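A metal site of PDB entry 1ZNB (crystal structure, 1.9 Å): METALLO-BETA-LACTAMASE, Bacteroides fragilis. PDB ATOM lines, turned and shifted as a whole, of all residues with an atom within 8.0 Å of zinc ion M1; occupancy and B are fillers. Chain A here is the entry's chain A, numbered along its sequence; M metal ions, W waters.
Zinc ion M1 is bound by water W1, a ring nitrogen (NE2) of His 206, the side-chain carboxylate of Asp 86, water W2 and the side-chain sulfur of Cys 164. Zinc ion M1 has five donor atoms within binding distance.
O of Pro 36 lies within hydrogen-bond range of ND1 of His 206 (2.8 Å).
Three residues have an atom within 4 Å of zinc ion M1: Asp 86, Cys 164 and His 206.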
ATOM      1  N   VAL A  35      32.876  22.850  25.424  1.00  0.00           N
ATOM      2  CA  VAL A  35      32.251  24.064  24.876  1.00  0.00           C
ATOM      3  C   VAL A  35      30.705  24.118  24.867  1.00  0.00           C
ATOM      4  O   VAL A  35      30.048  23.197  24.424  1.00  0.00           O
ATOM      5  CB  VAL A  35      32.690  24.182  23.398  1.00  0.00           C
ATOM      6  CG1 VAL A  35      32.119  25.431  22.718  1.00  0.00           C
ATOM      7  CG2 VAL A  35      34.195  24.076  23.318  1.00  0.00           C
ATOM      8  N   PRO A  36      30.131  25.217  25.338  1.00  0.00           N
ATOM      9  CA  PRO A  36      28.666  25.385  25.347  1.00  0.00           C
ATOM     10  C   PRO A  36      28.143  25.935  23.985  1.00  0.00           C
ATOM     11  O   PRO A  36      28.820  26.728  23.341  1.00  0.00           O
ATOM     12  CB  PRO A  36      28.466  26.391  26.454  1.00  0.00           C
ATOM     13  CG  PRO A  36      29.735  27.274  26.320  1.00  0.00           C
ATOM     14  CD  PRO A  36      30.784  26.209  26.216  1.00  0.00           C
ATOM     15  N   SER A  37      27.006  25.413  23.521  1.00  0.00           N
ATOM     16  CA  SER A  37      26.323  25.825  22.268  1.00  0.00           C
ATOM     17  C   SER A  37      24.866  26.191  22.604  1.00  0.00           C
ATOM     18  O   SER A  37      24.210  25.459  23.369  1.00  0.00           O
ATOM     19  CB  SER A  37      26.257  24.665  21.243  1.00  0.00           C
ATOM     20  OG  SER A  37      27.531  24.496  20.678  1.00  0.00           O
ATOM     21  N   ASN A  38      24.306  27.174  21.885  1.00  0.00           N
ATOM     22  CA  ASN A  38      22.918  27.610  22.151  1.00  0.00           C
ATOM     23  C   ASN A  38      21.961  27.287  21.015  1.00  0.00           C
ATOM     24  O   ASN A  38      22.359  27.254  19.810  1.00  0.00           O
ATOM     25  CB  ASN A  38      22.863  29.151  22.355  1.00  0.00           C
ATOM     26  CG  ASN A  38      23.712  29.623  23.496  1.00  0.00           C
ATOM     27  OD1 ASN A  38      23.964  28.882  24.413  1.00  0.00           O
ATOM     28  ND2 ASN A  38      24.179  30.888  23.426  1.00  0.00           N
ATOM     29  N   ASP A  52      18.441  25.263  15.731  1.00  0.00           N
ATOM     30  CA  ASP A  52      19.777  24.671  15.950  1.00  0.00           C
ATOM     31  C   ASP A  52      19.654  23.409  16.816  1.00  0.00           C
ATOM     32  O   ASP A  52      18.794  23.314  17.711  1.00  0.00           O
ATOM     33  CB  ASP A  52      20.721  25.656  16.666  1.00  0.00           C
ATOM     34  CG  ASP A  52      21.468  26.578  15.727  1.00  0.00           C
ATOM     35  OD1 ASP A  52      21.016  26.769  14.596  1.00  0.00           O
ATOM     36  OD2 ASP A  52      22.522  27.112  16.129  1.00  0.00           O
ATOM     37  N   ASN A  81      21.198  27.606  11.940  1.00  0.00           N
ATOM     38  CA  ASN A  81      21.796  28.894  11.697  1.00  0.00           C
ATOM     39  C   ASN A  81      22.791  28.863  10.527  1.00  0.00           C
ATOM     40  O   ASN A  81      22.887  29.823   9.728  1.00  0.00           O
ATOM     41  CB  ASN A  81      22.466  29.407  12.978  1.00  0.00           C
ATOM     42  CG  ASN A  81      22.899  30.813  12.838  1.00  0.00           C
ATOM     43  OD1 ASN A  81      24.062  31.060  12.499  1.00  0.00           O
ATOM     44  ND2 ASN A  81      21.948  31.757  13.020  1.00  0.00           N
ATOM     45  N   HIS A  82      23.603  27.802  10.497  1.00  0.00           N
ATOM     46  CA  HIS A  82      24.563  27.562   9.415  1.00  0.00           C
ATOM     47  C   HIS A  82      24.923  26.066   9.418  1.00  0.00           C
ATOM     48  O   HIS A  82      24.259  25.273  10.131  1.00  0.00           O
ATOM     49  CB  HIS A  82      25.775  28.506   9.484  1.00  0.00           C
ATOM     50  CG  HIS A  82      26.456  28.547  10.809  1.00  0.00           C
ATOM     51  ND1 HIS A  82      25.926  29.162  11.928  1.00  0.00           N
ATOM     52  CD2 HIS A  82      27.647  28.029  11.186  1.00  0.00           C
ATOM     53  CE1 HIS A  82      26.771  28.993  12.896  1.00  0.00           C
ATOM     54  NE2 HIS A  82      27.814  28.308  12.475  1.00  0.00           N
ATOM     55  N   HIS A  84      27.667  24.394  10.453  1.00  0.00           N
ATOM     56  CA  HIS A  84      28.492  23.828  11.536  1.00  0.00           C
ATOM     57  C   HIS A  84      27.735  22.839  12.453  1.00  0.00           C
ATOM     58  O   HIS A  84      26.496  22.871  12.524  1.00  0.00           O
ATOM     59  CB  HIS A  84      29.140  24.937  12.375  1.00  0.00           C
ATOM     60  CG  HIS A  84      30.272  25.600  11.669  1.00  0.00           C
ATOM     61  ND1 HIS A  84      30.770  26.829  12.019  1.00  0.00           N
ATOM     62  CD2 HIS A  84      31.019  25.178  10.626  1.00  0.00           C
ATOM     63  CE1 HIS A  84      31.781  27.143  11.229  1.00  0.00           C
ATOM     64  NE2 HIS A  84      31.955  26.155  10.371  1.00  0.00           N
ATOM     65  N   GLY A  85      28.508  21.957  13.104  1.00  0.00           N
ATOM     66  CA  GLY A  85      28.000  20.922  14.036  1.00  0.00           C
ATOM     67  C   GLY A  85      27.117  21.394  15.192  1.00  0.00           C
ATOM     68  O   GLY A  85      26.208  20.667  15.616  1.00  0.00           O
ATOM     69  N   ASP A  86      27.385  22.606  15.708  1.00  0.00           N
ATOM     70  CA  ASP A  86      26.576  23.219  16.779  1.00  0.00           C
ATOM     71  C   ASP A  86      25.249  23.838  16.185  1.00  0.00           C
ATOM     72  O   ASP A  86      24.509  24.545  16.873  1.00  0.00           O
ATOM     73  CB  ASP A  86      27.376  24.280  17.598  1.00  0.00           C
ATOM     74  CG  ASP A  86      28.040  25.359  16.736  1.00  0.00           C
ATOM     75  OD1 ASP A  86      28.674  25.085  15.692  1.00  0.00           O
ATOM     76  OD2 ASP A  86      27.901  26.526  17.122  1.00  0.00           O
ATOM     77  N   CYS A  87      24.949  23.517  14.927  1.00  0.00           N
ATOM     78  CA  CYS A  87      23.728  23.949  14.293  1.00  0.00           C
ATOM     79  C   CYS A  87      22.971  22.733  13.726  1.00  0.00           C
ATOM     80  O   CYS A  87      21.742  22.619  13.915  1.00  0.00           O
ATOM     81  CB  CYS A  87      23.965  24.948  13.162  1.00  0.00           C
ATOM     82  SG  CYS A  87      24.861  26.379  13.629  1.00  0.00           S
ATOM     83  N   HIS A 145      30.116  35.134  10.633  1.00  0.00           N
ATOM     84  CA  HIS A 145      30.814  34.018  11.263  1.00  0.00           C
ATOM     85  C   HIS A 145      31.002  32.819  10.248  1.00  0.00           C
ATOM     86  O   HIS A 145      32.012  32.123  10.260  1.00  0.00           O
ATOM     87  CB  HIS A 145      29.996  33.540  12.484  1.00  0.00           C
ATOM     88  CG  HIS A 145      30.335  32.130  12.869  1.00  0.00           C
ATOM     89  ND1 HIS A 145      31.435  31.820  13.632  1.00  0.00           N
ATOM     90  CD2 HIS A 145      29.748  30.967  12.547  1.00  0.00           C
ATOM     91  CE1 HIS A 145      31.508  30.515  13.781  1.00  0.00           C
ATOM     92  NE2 HIS A 145      30.502  29.971  13.123  1.00  0.00           N
ATOM     93  N   GLY A 163      22.300  33.750  16.451  1.00  0.00           N
ATOM     94  CA  GLY A 163      23.254  32.693  16.175  1.00  0.00           C
ATOM     95  C   GLY A 163      24.733  33.121  16.310  1.00  0.00           C
ATOM     96  O   GLY A 163      25.007  34.194  16.854  1.00  0.00           O
ATOM     97  N   CYS A 164      25.642  32.309  15.770  1.00  0.00           N
ATOM     98  CA  CYS A 164      27.101  32.494  15.904  1.00  0.00           C
ATOM     99  C   CYS A 164      27.703  33.770  15.324  1.00  0.00           C
ATOM    100  O   CYS A 164      28.818  34.124  15.657  1.00  0.00           O
ATOM    101  CB  CYS A 164      27.824  31.256  15.441  1.00  0.00           C
ATOM    102  SG  CYS A 164      27.263  29.746  16.260  1.00  0.00           S
ATOM    103  N   MET A 165      26.970  34.467  14.463  1.00  0.00           N
ATOM    104  CA  MET A 165      27.457  35.739  13.945  1.00  0.00           C
ATOM    105  C   MET A 165      27.471  36.762  15.156  1.00  0.00           C
ATOM    106  O   MET A 165      28.104  37.813  15.103  1.00  0.00           O
ATOM    107  CB  MET A 165      26.530  36.241  12.853  1.00  0.00           C
ATOM    108  CG  MET A 165      25.185  36.906  13.370  1.00  0.00           C
ATOM    109  SD  MET A 165      24.426  37.832  12.030  1.00  0.00           S
ATOM    110  CE  MET A 165      23.924  36.406  10.919  1.00  0.00           C
ATOM    111  N   LEU A 166      26.776  36.425  16.260  1.00  0.00           N
ATOM    112  CA  LEU A 166      26.716  37.307  17.462  1.00  0.00           C
ATOM    113  C   LEU A 166      27.514  36.693  18.590  1.00  0.00           C
ATOM    114  O   LEU A 166      27.453  35.481  18.777  1.00  0.00           O
ATOM    115  CB  LEU A 166      25.268  37.499  17.937  1.00  0.00           C
ATOM    116  CG  LEU A 166      24.328  38.170  16.927  1.00  0.00           C
ATOM    117  CD1 LEU A 166      23.025  38.468  17.620  1.00  0.00           C
ATOM    118  CD2 LEU A 166      24.939  39.471  16.389  1.00  0.00           C
ATOM    119  N   LYS A 167      28.289  37.509  19.305  1.00  0.00           N
ATOM    120  CA  LYS A 167      29.096  37.061  20.454  1.00  0.00           C
ATOM    121  C   LYS A 167      28.392  37.592  21.739  1.00  0.00           C
ATOM    122  O   LYS A 167      27.756  38.659  21.692  1.00  0.00           O
ATOM    123  CB  LYS A 167      30.517  37.719  20.406  1.00  0.00           C
ATOM    124  CG  LYS A 167      31.435  37.382  19.214  1.00  0.00           C
ATOM    125  CD  LYS A 167      31.961  36.031  19.372  1.00  0.00           C
ATOM    126  CE  LYS A 167      32.780  35.662  18.217  1.00  0.00           C
ATOM    127  NZ  LYS A 167      33.393  34.421  18.698  1.00  0.00           N
ATOM    128  N   ASN A 176      36.656  31.056  15.825  1.00  0.00           N
ATOM    129  CA  ASN A 176      36.858  30.275  14.603  1.00  0.00           C
ATOM    130  C   ASN A 176      36.419  31.064  13.389  1.00  0.00           C
ATOM    131  O   ASN A 176      35.245  31.280  13.214  1.00  0.00           O
ATOM    132  CB  ASN A 176      36.020  28.989  14.722  1.00  0.00           C
ATOM    133  CG  ASN A 176      35.987  28.191  13.415  1.00  0.00           C
ATOM    134  OD1 ASN A 176      36.943  28.237  12.617  1.00  0.00           O
ATOM    135  ND2 ASN A 176      34.898  27.436  13.197  1.00  0.00           N
ATOM    136  N   PRO A 204      22.899  34.737  21.217  1.00  0.00           N
ATOM    137  CA  PRO A 204      24.093  34.456  20.390  1.00  0.00           C
ATOM    138  C   PRO A 204      24.284  32.937  20.169  1.00  0.00           C
ATOM    139  O   PRO A 204      23.518  32.140  20.745  1.00  0.00           O
ATOM    140  CB  PRO A 204      25.253  35.081  21.221  1.00  0.00           C
ATOM    141  CG  PRO A 204      24.832  34.732  22.636  1.00  0.00           C
ATOM    142  CD  PRO A 204      23.285  35.007  22.636  1.00  0.00           C
ATOM    143  N   GLY A 205      25.258  32.567  19.307  1.00  0.00           N
ATOM    144  CA  GLY A 205      25.533  31.159  19.064  1.00  0.00           C
ATOM    145  C   GLY A 205      26.115  30.430  20.278  1.00  0.00           C
ATOM    146  O   GLY A 205      25.881  29.229  20.495  1.00  0.00           O
ATOM    147  N   HIS A 206      26.895  31.173  21.053  1.00  0.00           N
ATOM    148  CA  HIS A 206      27.543  30.705  22.278  1.00  0.00           C
ATOM    149  C   HIS A 206      27.533  31.795  23.366  1.00  0.00           C
ATOM    150  O   HIS A 206      27.767  32.976  23.085  1.00  0.00           O
ATOM    151  CB  HIS A 206      28.988  30.313  21.970  1.00  0.00           C
ATOM    152  CG  HIS A 206      29.133  29.404  20.790  1.00  0.00           C
ATOM    153  ND1 HIS A 206      29.103  28.031  20.905  1.00  0.00           N
ATOM    154  CD2 HIS A 206      29.268  29.670  19.479  1.00  0.00           C
ATOM    155  CE1 HIS A 206      29.223  27.495  19.708  1.00  0.00           C
ATOM    156  NE2 HIS A 206      29.333  28.470  18.827  1.00  0.00           N
HETATM  157 ZN    ZN M   1      29.064  28.404  16.739  1.00  0.00          ZN
HETATM  158 ZN    ZN M   2      29.756  28.053  13.359  1.00  0.00          ZN
HETATM  159  O   HOH W   1      29.881  27.422  15.123  1.00  0.00           O
HETATM  160  O   HOH W   2      30.729  29.946  16.765  1.00  0.00           O
